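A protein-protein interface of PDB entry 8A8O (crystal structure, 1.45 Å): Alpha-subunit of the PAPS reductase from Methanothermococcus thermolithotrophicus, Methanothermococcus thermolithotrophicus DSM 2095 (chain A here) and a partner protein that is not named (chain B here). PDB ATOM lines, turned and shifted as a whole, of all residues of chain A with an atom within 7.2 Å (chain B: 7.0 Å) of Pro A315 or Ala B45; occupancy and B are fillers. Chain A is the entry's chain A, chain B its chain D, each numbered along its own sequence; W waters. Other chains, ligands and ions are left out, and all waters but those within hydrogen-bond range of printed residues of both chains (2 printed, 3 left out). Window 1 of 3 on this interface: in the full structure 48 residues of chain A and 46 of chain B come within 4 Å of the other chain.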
ATOM      1  N   ARG A  45       0.392  15.585  11.819  1.00  0.00           N
ATOM      2  CA  ARG A  45       1.123  14.437  11.302  1.00  0.00           C
ATOM      3  C   ARG A  45       2.019  14.762  10.111  1.00  0.00           C
ATOM      4  O   ARG A  45       2.557  13.841   9.494  1.00  0.00           O
ATOM      5  CB  ARG A  45       0.149  13.323  10.866  1.00  0.00           C
ATOM      6  CG  ARG A  45      -0.513  12.594  11.995  1.00  0.00           C
ATOM      7  CD  ARG A  45       0.388  11.502  12.550  1.00  0.00           C
ATOM      8  NE  ARG A  45      -0.333  10.720  13.551  1.00  0.00           N
ATOM      9  CZ  ARG A  45       0.217   9.777  14.308  1.00  0.00           C
ATOM     10  NH1 ARG A  45       1.477   9.417  14.152  1.00  0.00           N
ATOM     11  NH2 ARG A  45      -0.523   9.180  15.235  1.00  0.00           N
ATOM     12  N   ALA A  50       5.429  11.364   9.947  1.00  0.00           N
ATOM     13  CA  ALA A  50       4.012  11.024   9.969  1.00  0.00           C
ATOM     14  C   ALA A  50       3.734   9.647  10.547  1.00  0.00           C
ATOM     15  O   ALA A  50       2.791   9.484  11.322  1.00  0.00           O
ATOM     16  CB  ALA A  50       3.419  11.134   8.563  1.00  0.00           C
ATOM     17  N   ALA A  51       4.526   8.641  10.172  1.00  0.00           N
ATOM     18  CA  ALA A  51       4.266   7.274  10.588  1.00  0.00           C
ATOM     19  C   ALA A  51       4.866   6.939  11.945  1.00  0.00           C
ATOM     20  O   ALA A  51       4.620   5.840  12.455  1.00  0.00           O
ATOM     21  CB  ALA A  51       4.843   6.284   9.564  1.00  0.00           C
ATOM     22  N   GLU A 128       5.788   6.503  18.024  1.00  0.00           N
ATOM     23  CA  GLU A 128       4.599   6.470  17.181  1.00  0.00           C
ATOM     24  C   GLU A 128       3.947   7.839  17.069  1.00  0.00           C
ATOM     25  O   GLU A 128       3.459   8.209  15.997  1.00  0.00           O
ATOM     26  CB  GLU A 128       3.584   5.471  17.731  1.00  0.00           C
ATOM     27  CG  GLU A 128       2.321   5.360  16.881  1.00  0.00           C
ATOM     28  CD  GLU A 128       1.251   6.408  17.209  1.00  0.00           C
ATOM     29  OE1 GLU A 128       1.120   6.795  18.393  1.00  0.00           O
ATOM     30  OE2 GLU A 128       0.545   6.849  16.271  1.00  0.00           O
ATOM     31  N   VAL A 241       8.246  -2.556   1.222  1.00  0.00           N
ATOM     32  CA  VAL A 241       7.612  -1.752   2.260  1.00  0.00           C
ATOM     33  C   VAL A 241       8.510  -0.616   2.726  1.00  0.00           C
ATOM     34  O   VAL A 241       8.014   0.336   3.344  1.00  0.00           O
ATOM     35  CB  VAL A 241       7.186  -2.655   3.423  1.00  0.00           C
ATOM     36  CG1 VAL A 241       5.970  -3.495   3.015  1.00  0.00           C
ATOM     37  CG2 VAL A 241       8.341  -3.543   3.861  1.00  0.00           C
ATOM     38  N   SER A 243      10.785  -0.327   4.999  1.00  0.00           N
ATOM     39  CA  SER A 243      10.739  -0.155   6.434  1.00  0.00           C
ATOM     40  C   SER A 243      12.129   0.009   7.027  1.00  0.00           C
ATOM     41  O   SER A 243      13.122  -0.442   6.448  1.00  0.00           O
ATOM     42  CB  SER A 243      10.081  -1.381   7.067  1.00  0.00           C
ATOM     43  OG  SER A 243       8.815  -1.627   6.471  1.00  0.00           O
ATOM     44  N   LYS A 307       7.179  -6.990  15.943  1.00  0.00           N
ATOM     45  CA  LYS A 307       5.883  -6.639  15.374  1.00  0.00           C
ATOM     46  C   LYS A 307       5.324  -5.383  16.030  1.00  0.00           C
ATOM     47  O   LYS A 307       4.794  -4.496  15.347  1.00  0.00           O
ATOM     48  CB  LYS A 307       4.921  -7.809  15.558  1.00  0.00           C
ATOM     49  CG  LYS A 307       5.219  -8.976  14.652  1.00  0.00           C
ATOM     50  CD  LYS A 307       4.645 -10.265  15.180  1.00  0.00           C
ATOM     51  CE  LYS A 307       3.143 -10.340  15.000  1.00  0.00           C
ATOM     52  NZ  LYS A 307       2.685 -11.773  15.085  1.00  0.00           N
ATOM     53  N   ALA A 309       7.048  -2.984  17.512  1.00  0.00           N
ATOM     54  CA  ALA A 309       7.870  -1.853  17.103  1.00  0.00           C
ATOM     55  C   ALA A 309       7.509  -1.391  15.697  1.00  0.00           C
ATOM     56  O   ALA A 309       7.309  -0.198  15.455  1.00  0.00           O
ATOM     57  CB  ALA A 309       9.352  -2.229  17.191  1.00  0.00           C
ATOM     58  N   TYR A 310       7.409  -2.323  14.749  1.00  0.00           N
ATOM     59  CA  TYR A 310       7.111  -1.920  13.377  1.00  0.00           C
ATOM     60  C   TYR A 310       5.681  -1.408  13.233  1.00  0.00           C
ATOM     61  O   TYR A 310       5.420  -0.540  12.390  1.00  0.00           O
ATOM     62  CB  TYR A 310       7.364  -3.097  12.439  1.00  0.00           C
ATOM     63  CG  TYR A 310       8.803  -3.219  12.007  1.00  0.00           C
ATOM     64  CD1 TYR A 310       9.435  -2.201  11.329  1.00  0.00           C
ATOM     65  CD2 TYR A 310       9.539  -4.348  12.309  1.00  0.00           C
ATOM     66  CE1 TYR A 310      10.750  -2.304  10.938  1.00  0.00           C
ATOM     67  CE2 TYR A 310      10.858  -4.461  11.927  1.00  0.00           C
ATOM     68  CZ  TYR A 310      11.458  -3.429  11.246  1.00  0.00           C
ATOM     69  OH  TYR A 310      12.770  -3.518  10.858  1.00  0.00           O
ATOM     70  N   LEU A 311       4.737  -1.933  14.016  1.00  0.00           N
ATOM     71  CA  LEU A 311       3.397  -1.354  13.996  1.00  0.00           C
ATOM     72  C   LEU A 311       3.448   0.116  14.377  1.00  0.00           C
ATOM     73  O   LEU A 311       2.668   0.924  13.863  1.00  0.00           O
ATOM     74  CB  LEU A 311       2.450  -2.119  14.913  1.00  0.00           C
ATOM     75  CG  LEU A 311       1.986  -3.474  14.368  1.00  0.00           C
ATOM     76  CD1 LEU A 311       1.369  -4.291  15.472  1.00  0.00           C
ATOM     77  CD2 LEU A 311       1.005  -3.280  13.205  1.00  0.00           C
ATOM     78  N   SER A 312       4.397   0.488  15.224  1.00  0.00           N
ATOM     79  CA  SER A 312       4.508   1.846  15.734  1.00  0.00           C
ATOM     80  C   SER A 312       5.296   2.788  14.836  1.00  0.00           C
ATOM     81  O   SER A 312       5.449   3.967  15.194  1.00  0.00           O
ATOM     82  CB  SER A 312       5.149   1.811  17.118  1.00  0.00           C
ATOM     83  OG  SER A 312       4.408   0.970  17.983  1.00  0.00           O
ATOM     84  N   MET A 313       5.803   2.322  13.691  1.00  0.00           N
ATOM     85  CA  MET A 313       6.539   3.224  12.816  1.00  0.00           C
ATOM     86  C   MET A 313       6.605   2.835  11.350  1.00  0.00           C
ATOM     87  O   MET A 313       6.939   3.681  10.520  1.00  0.00           O
ATOM     88  CB  MET A 313       7.952   3.501  13.381  1.00  0.00           C
ATOM     89  CG  MET A 313       8.692   2.287  13.895  1.00  0.00           C
ATOM     90  SD  MET A 313       9.535   1.413  12.601  1.00  0.00           S
ATOM     91  CE  MET A 313      10.447   0.182  13.523  1.00  0.00           C
ATOM     92  N   SER A 314       6.267   1.595  11.002  1.00  0.00           N
ATOM     93  CA  SER A 314       6.224   1.199   9.593  1.00  0.00           C
ATOM     94  C   SER A 314       5.281   0.016   9.433  1.00  0.00           C
ATOM     95  O   SER A 314       5.732  -1.116   9.194  1.00  0.00           O
ATOM     96  CB  SER A 314       7.630   0.845   9.103  1.00  0.00           C
ATOM     97  OG  SER A 314       7.706   0.806   7.688  1.00  0.00           O
ATOM     98  N   PRO A 315       3.970   0.234   9.561  1.00  0.00           N
ATOM     99  CA  PRO A 315       3.043  -0.906   9.676  1.00  0.00           C
ATOM    100  C   PRO A 315       2.973  -1.782   8.442  1.00  0.00           C
ATOM    101  O   PRO A 315       2.595  -2.957   8.570  1.00  0.00           O
ATOM    102  CB  PRO A 315       1.681  -0.235   9.927  1.00  0.00           C
ATOM    103  CG  PRO A 315       2.018   1.124  10.434  1.00  0.00           C
ATOM    104  CD  PRO A 315       3.284   1.527   9.760  1.00  0.00           C
ATOM    105  N   GLY A 316       3.319  -1.259   7.265  1.00  0.00           N
ATOM    106  CA  GLY A 316       3.222  -2.050   6.048  1.00  0.00           C
ATOM    107  C   GLY A 316       3.969  -3.366   6.110  1.00  0.00           C
ATOM    108  O   GLY A 316       3.568  -4.340   5.469  1.00  0.00           O
ATOM    109  N   ILE A 317       5.082  -3.413   6.847  1.00  0.00           N
ATOM    110  CA  ILE A 317       5.868  -4.651   6.905  1.00  0.00           C
ATOM    111  C   ILE A 317       5.064  -5.794   7.511  1.00  0.00           C
ATOM    112  O   ILE A 317       5.232  -6.963   7.121  1.00  0.00           O
ATOM    113  CB  ILE A 317       7.204  -4.416   7.640  1.00  0.00           C
ATOM    114  CG1 ILE A 317       8.167  -5.577   7.370  1.00  0.00           C
ATOM    115  CG2 ILE A 317       7.003  -4.281   9.125  1.00  0.00           C
ATOM    116  CD1 ILE A 317       9.612  -5.279   7.801  1.00  0.00           C
ATOM    117  N   ILE A 318       4.191  -5.495   8.476  1.00  0.00           N
ATOM    118  CA  ILE A 318       3.373  -6.542   9.080  1.00  0.00           C
ATOM    119  C   ILE A 318       2.494  -7.186   8.021  1.00  0.00           C
ATOM    120  O   ILE A 318       2.291  -8.407   8.012  1.00  0.00           O
ATOM    121  CB  ILE A 318       2.543  -5.974  10.249  1.00  0.00           C
ATOM    122  CG1 ILE A 318       3.456  -5.365  11.320  1.00  0.00           C
ATOM    123  CG2 ILE A 318       1.669  -7.044  10.858  1.00  0.00           C
ATOM    124  CD1 ILE A 318       4.562  -6.297  11.797  1.00  0.00           C
ATOM    125  N   LEU A 319       1.990  -6.384   7.089  1.00  0.00           N
ATOM    126  CA  LEU A 319       1.131  -6.930   6.040  1.00  0.00           C
ATOM    127  C   LEU A 319       1.933  -7.783   5.071  1.00  0.00           C
ATOM    128  O   LEU A 319       1.460  -8.833   4.632  1.00  0.00           O
ATOM    129  CB  LEU A 319       0.443  -5.790   5.310  1.00  0.00           C
ATOM    130  CG  LEU A 319      -0.569  -5.013   6.152  1.00  0.00           C
ATOM    131  CD1 LEU A 319      -1.097  -3.834   5.368  1.00  0.00           C
ATOM    132  CD2 LEU A 319      -1.702  -5.938   6.571  1.00  0.00           C
ATOM    133  N   LYS A 320       3.145  -7.348   4.721  1.00  0.00           N
ATOM    134  CA  LYS A 320       3.989  -8.162   3.861  1.00  0.00           C
ATOM    135  C   LYS A 320       4.288  -9.499   4.507  1.00  0.00           C
ATOM    136  O   LYS A 320       4.215 -10.548   3.852  1.00  0.00           O
ATOM    137  CB  LYS A 320       5.289  -7.428   3.553  1.00  0.00           C
ATOM    138  CG  LYS A 320       6.202  -8.212   2.625  1.00  0.00           C
ATOM    139  CD  LYS A 320       7.516  -7.476   2.398  1.00  0.00           C
ATOM    140  CE  LYS A 320       8.552  -8.371   1.724  1.00  0.00           C
ATOM    141  NZ  LYS A 320       8.371  -8.415   0.244  1.00  0.00           N
ATOM    142  N   ILE B   3      -4.717   2.371   1.317  1.00  0.00           N
ATOM    143  CA  ILE B   3      -5.868   2.233   2.202  1.00  0.00           C
ATOM    144  C   ILE B   3      -7.158   2.201   1.396  1.00  0.00           C
ATOM    145  O   ILE B   3      -7.233   2.673   0.265  1.00  0.00           O
ATOM    146  CB  ILE B   3      -5.939   3.331   3.291  1.00  0.00           C
ATOM    147  CG1 ILE B   3      -6.103   4.711   2.651  1.00  0.00           C
ATOM    148  CG2 ILE B   3      -4.723   3.260   4.179  1.00  0.00           C
ATOM    149  CD1 ILE B   3      -7.494   5.204   2.536  1.00  0.00           C
ATOM    150  N   VAL B  19      -5.613  14.595   8.873  1.00  0.00           N
ATOM    151  CA  VAL B  19      -4.358  14.022   9.356  1.00  0.00           C
ATOM    152  C   VAL B  19      -3.360  13.716   8.239  1.00  0.00           C
ATOM    153  O   VAL B  19      -2.147  13.692   8.478  1.00  0.00           O
ATOM    154  CB  VAL B  19      -4.604  12.755  10.214  1.00  0.00           C
ATOM    155  CG1 VAL B  19      -5.490  13.060  11.415  1.00  0.00           C
ATOM    156  CG2 VAL B  19      -5.206  11.622   9.368  1.00  0.00           C
ATOM    157  N   CYS B  41      -0.777   6.979  -1.682  1.00  0.00           N
ATOM    158  CA  CYS B  41      -0.670   6.684  -0.262  1.00  0.00           C
ATOM    159  C   CYS B  41       0.726   6.187   0.108  1.00  0.00           C
ATOM    160  O   CYS B  41       1.329   5.362  -0.596  1.00  0.00           O
ATOM    161  CB  CYS B  41      -1.737   5.660   0.146  1.00  0.00           C
ATOM    162  SG  CYS B  41      -1.740   5.207   1.880  1.00  0.00           S
ATOM    163  N   TRP B  42       1.246   6.726   1.219  1.00  0.00           N
ATOM    164  CA  TRP B  42       2.544   6.385   1.798  1.00  0.00           C
ATOM    165  C   TRP B  42       2.461   5.297   2.868  1.00  0.00           C
ATOM    166  O   TRP B  42       3.500   4.888   3.393  1.00  0.00           O
ATOM    167  CB  TRP B  42       3.136   7.671   2.410  1.00  0.00           C
ATOM    168  CG  TRP B  42       4.589   7.642   2.829  1.00  0.00           C
ATOM    169  CD1 TRP B  42       5.591   6.875   2.306  1.00  0.00           C
ATOM    170  CD2 TRP B  42       5.200   8.463   3.836  1.00  0.00           C
ATOM    171  NE1 TRP B  42       6.787   7.168   2.935  1.00  0.00           N
ATOM    172  CE2 TRP B  42       6.568   8.137   3.874  1.00  0.00           C
ATOM    173  CE3 TRP B  42       4.720   9.449   4.698  1.00  0.00           C
ATOM    174  CZ2 TRP B  42       7.459   8.750   4.756  1.00  0.00           C
ATOM    175  CZ3 TRP B  42       5.609  10.050   5.585  1.00  0.00           C
ATOM    176  CH2 TRP B  42       6.951   9.706   5.604  1.00  0.00           C
ATOM    177  N   ASP B  43       1.259   4.823   3.217  1.00  0.00           N
ATOM    178  CA  ASP B  43       1.076   3.807   4.243  1.00  0.00           C
ATOM    179  C   ASP B  43       1.585   4.261   5.609  1.00  0.00           C
ATOM    180  O   ASP B  43       2.078   3.458   6.409  1.00  0.00           O
ATOM    181  CB  ASP B  43       1.665   2.461   3.848  1.00  0.00           C
ATOM    182  CG  ASP B  43       0.899   1.802   2.742  1.00  0.00           C
ATOM    183  OD1 ASP B  43      -0.352   1.752   2.875  1.00  0.00           O
ATOM    184  OD2 ASP B  43       1.522   1.368   1.747  1.00  0.00           O
ATOM    185  N   CYS B  44       1.418   5.556   5.915  1.00  0.00           N
ATOM    186  CA  CYS B  44       1.810   6.055   7.228  1.00  0.00           C
ATOM    187  C   CYS B  44       0.839   5.656   8.339  1.00  0.00           C
ATOM    188  O   CYS B  44       1.187   5.785   9.510  1.00  0.00           O
ATOM    189  CB  CYS B  44       1.950   7.583   7.185  1.00  0.00           C
ATOM    190  SG  CYS B  44       0.398   8.511   7.205  1.00  0.00           S
ATOM    191  N   ALA B  45      -0.386   5.235   7.997  1.00  0.00           N
ATOM    192  CA  ALA B  45      -1.435   4.774   8.905  1.00  0.00           C
ATOM    193  C   ALA B  45      -2.075   5.861   9.763  1.00  0.00           C
ATOM    194  O   ALA B  45      -2.855   5.539  10.666  1.00  0.00           O
ATOM    195  CB  ALA B  45      -0.988   3.581   9.770  1.00  0.00           C
ATOM    196  N   ALA B  46      -1.824   7.137   9.492  1.00  0.00           N
ATOM    197  CA  ALA B  46      -2.391   8.182  10.340  1.00  0.00           C
ATOM    198  C   ALA B  46      -3.912   8.152  10.281  1.00  0.00           C
ATOM    199  O   ALA B  46      -4.583   8.241  11.309  1.00  0.00           O
ATOM    200  CB  ALA B  46      -1.868   9.551   9.911  1.00  0.00           C
ATOM    201  N   CYS B  47      -4.460   7.952   9.075  1.00  0.00           N
ATOM    202  CA  CYS B  47      -5.909   7.870   8.902  1.00  0.00           C
ATOM    203  C   CYS B  47      -6.486   6.606   9.534  1.00  0.00           C
ATOM    204  O   CYS B  47      -7.552   6.655  10.158  1.00  0.00           O
ATOM    205  CB  CYS B  47      -6.235   7.941   7.409  1.00  0.00           C
ATOM    206  SG  CYS B  47      -5.493   6.620   6.430  1.00  0.00           S
ATOM    207  N   VAL B  48      -5.809   5.471   9.356  1.00  0.00           N
ATOM    208  CA  VAL B  48      -6.265   4.213   9.931  1.00  0.00           C
ATOM    209  C   VAL B  48      -6.460   4.368  11.432  1.00  0.00           C
ATOM    210  O   VAL B  48      -7.465   3.921  12.003  1.00  0.00           O
ATOM    211  CB  VAL B  48      -5.266   3.087   9.605  1.00  0.00           C
ATOM    212  CG1 VAL B  48      -5.723   1.779  10.242  1.00  0.00           C
ATOM    213  CG2 VAL B  48      -5.078   2.936   8.099  1.00  0.00           C
ATOM    214  N   LYS B  49      -5.490   5.003  12.094  1.00  0.00           N
ATOM    215  CA  LYS B  49      -5.577   5.191  13.536  1.00  0.00           C
ATOM    216  C   LYS B  49      -6.671   6.183  13.912  1.00  0.00           C
ATOM    217  O   LYS B  49      -7.305   6.039  14.961  1.00  0.00           O
ATOM    218  CB  LYS B  49      -4.246   5.707  14.087  1.00  0.00           C
ATOM    219  CG  LYS B  49      -3.090   4.758  13.944  1.00  0.00           C
ATOM    220  CD  LYS B  49      -1.789   5.525  14.211  1.00  0.00           C
ATOM    221  CE  LYS B  49      -0.599   4.924  13.526  1.00  0.00           C
ATOM    222  NZ  LYS B  49       0.619   5.755  13.750  1.00  0.00           N
ATOM    223  N   GLU B  50      -6.893   7.194  13.079  1.00  0.00           N
ATOM    224  CA  GLU B  50      -7.834   8.251  13.415  1.00  0.00           C
ATOM    225  C   GLU B  50      -9.285   7.783  13.364  1.00  0.00           C
ATOM    226  O   GLU B  50     -10.121   8.302  14.110  1.00  0.00           O
ATOM    227  CB  GLU B  50      -7.631   9.408  12.437  1.00  0.00           C
ATOM    228  CG  GLU B  50      -8.284  10.696  12.857  1.00  0.00           C
ATOM    229  CD  GLU B  50      -7.637  11.287  14.094  1.00  0.00           C
ATOM    230  OE1 GLU B  50      -6.605  10.739  14.551  1.00  0.00           O
ATOM    231  OE2 GLU B  50      -8.168  12.296  14.599  1.00  0.00           O
ATOM    232  N   MET B  58      -5.785  -0.673   5.928  1.00  0.00           N
ATOM    233  CA  MET B  58      -4.599  -0.631   5.081  1.00  0.00           C
ATOM    234  C   MET B  58      -4.404  -2.017   4.486  1.00  0.00           C
ATOM    235  O   MET B  58      -4.671  -3.028   5.146  1.00  0.00           O
ATOM    236  CB  MET B  58      -3.386  -0.256   5.937  1.00  0.00           C
ATOM    237  CG  MET B  58      -2.048  -0.353   5.233  1.00  0.00           C
ATOM    238  SD  MET B  58      -0.676   0.283   6.206  1.00  0.00           S
ATOM    239  CE  MET B  58      -1.190   1.968   6.474  1.00  0.00           C
ATOM    240  N   LEU B  60      -1.753  -4.061   1.266  1.00  0.00           N
ATOM    241  CA  LEU B  60      -0.675  -3.878   0.291  1.00  0.00           C
ATOM    242  C   LEU B  60      -1.219  -4.036  -1.125  1.00  0.00           C
ATOM    243  O   LEU B  60      -2.012  -4.943  -1.405  1.00  0.00           O
ATOM    244  CB  LEU B  60       0.434  -4.900   0.534  1.00  0.00           C
ATOM    245  CG  LEU B  60       1.277  -4.630   1.775  1.00  0.00           C
ATOM    246  CD1 LEU B  60       2.402  -5.654   1.820  1.00  0.00           C
ATOM    247  CD2 LEU B  60       1.826  -3.218   1.804  1.00  0.00           C
ATOM    248  N   LEU B  71      -4.938  -4.228   7.813  1.00  0.00           N
ATOM    249  CA  LEU B  71      -4.633  -3.658   9.117  1.00  0.00           C
ATOM    250  C   LEU B  71      -5.678  -2.595   9.424  1.00  0.00           C
ATOM    251  O   LEU B  71      -5.959  -1.736   8.578  1.00  0.00           O
ATOM    252  CB  LEU B  71      -3.264  -2.984   9.054  1.00  0.00           C
ATOM    253  CG  LEU B  71      -2.044  -3.604   9.712  1.00  0.00           C
ATOM    254  CD1 LEU B  71      -0.854  -2.663   9.564  1.00  0.00           C
ATOM    255  CD2 LEU B  71      -2.332  -3.886  11.167  1.00  0.00           C
ATOM    256  N   ALA B  73      -6.969  -0.105  13.069  1.00  0.00           N
ATOM    257  CA  ALA B  73      -6.437   0.360  14.344  1.00  0.00           C
ATOM    258  C   ALA B  73      -7.484   1.118  15.144  1.00  0.00           C
ATOM    259  O   ALA B  73      -8.210   1.956  14.612  1.00  0.00           O
ATOM    260  CB  ALA B  73      -5.216   1.274  14.142  1.00  0.00           C
ATOM    261  N   TRP B  82      -4.184  -2.744  17.397  1.00  0.00           N
ATOM    262  CA  TRP B  82      -4.064  -3.073  15.986  1.00  0.00           C
ATOM    263  C   TRP B  82      -4.774  -4.383  15.698  1.00  0.00           C
ATOM    264  O   TRP B  82      -4.594  -5.364  16.433  1.00  0.00           O
ATOM    265  CB  TRP B  82      -2.594  -3.230  15.604  1.00  0.00           C
ATOM    266  CG  TRP B  82      -1.801  -1.961  15.688  1.00  0.00           C
ATOM    267  CD1 TRP B  82      -1.086  -1.506  16.754  1.00  0.00           C
ATOM    268  CD2 TRP B  82      -1.653  -0.985  14.655  1.00  0.00           C
ATOM    269  NE1 TRP B  82      -0.486  -0.304  16.441  1.00  0.00           N
ATOM    270  CE2 TRP B  82      -0.828   0.039  15.161  1.00  0.00           C
ATOM    271  CE3 TRP B  82      -2.138  -0.875  13.352  1.00  0.00           C
ATOM    272  CZ2 TRP B  82      -0.479   1.164  14.401  1.00  0.00           C
ATOM    273  CZ3 TRP B  82      -1.783   0.238  12.604  1.00  0.00           C
ATOM    274  CH2 TRP B  82      -0.962   1.233  13.132  1.00  0.00           C
HETATM  275  O   HOH W   1       1.473   1.377  17.875  1.00  0.00           O
HETATM  276  O   HOH W   2       4.110   1.399   6.371  1.00  0.00           O
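Ala B45 touches one residue of chain A.
Of the printed residues of chain B, Lys A320 touches Leu B60 (3.4 Å).
Printed residues of chain B within 4 Å of Leu A311: Leu B71 (3.96 Å) and Trp B82 (3.2 Å).
The nearest printed residue of chain B that does not touch Pro A315 is Trp B82 (4.02 Å).
The nearest printed residue of chain B that does not touch Glu A128 is Trp B82 (5.6 Å).
NZ of Lys B49 is in salt-bridge range of OE2 of Glu A128 (2.7 Å).
Of the 19 printed residues of chain A, 8 touch a printed residue of chain B.
Printed residues of chain A that touch a printed residue of chain B: Arg A45, Ala A50, Ala A51, Glu A128, Leu A311, Pro A315, Leu A319 and Lys A320.
Hydrophobic or aromatic side chains of chain A within 4 Å of the printed part of chain B: Ala A50, Ala A51, Leu A311, Pro A315 and Leu A319.
Hydrophobic or aromatic side chains of chain B within 4 Å of the printed part of chain A: Trp B42, Ala B45, Ala B46, Met B58, Leu B60, Leu B71 and Trp B82.
Among the printed residues, 14 pairs touch across the chains.
Water W2 bridges O of Asp B43 (2.9 Å) and N of Gly A316 (2.9 Å).
Water W1 bridges NE1 of Trp B82 (3.0 Å) and OG of Ser A312 (3.0 Å).
O of Ala A50 is in hydrogen-bond range of NH1 of Arg A45 (3.1 Å).
The guanidinium group (NH2) of Arg A45 lies within salt-bridge range of the side-chain carboxylate (OE2) of Glu A128, at 2.8 Å.
The side-chain sulfur (SG) of Cys B44 lies close to the backbone NH (N) of Ala B46, 3.5 Å away.
The backbone carbonyl oxygen of Leu B71 is in hydrogen-bond range of the backbone NH of Met B58.
Arg A45 touches Val B19 (CB to O, 3.3 Å).
NZ of Lys B49 touches NH1 of Arg A45, at 3.8 Å.
Ala A50 touches Trp B42 (CB to CZ3, 3.9 Å).
O of Cys B44 touches CA of Ala A51, at 3.6 Å.
Leu B71 touches Leu A311.
Ala B45 touches Pro A315.
Pro A315 touches Leu B71.
Met B58 touches Leu A319 (CG to CD1, 3.6 Å).
Leu A319 touches Leu B60.
Leu A319 touches Leu B71.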
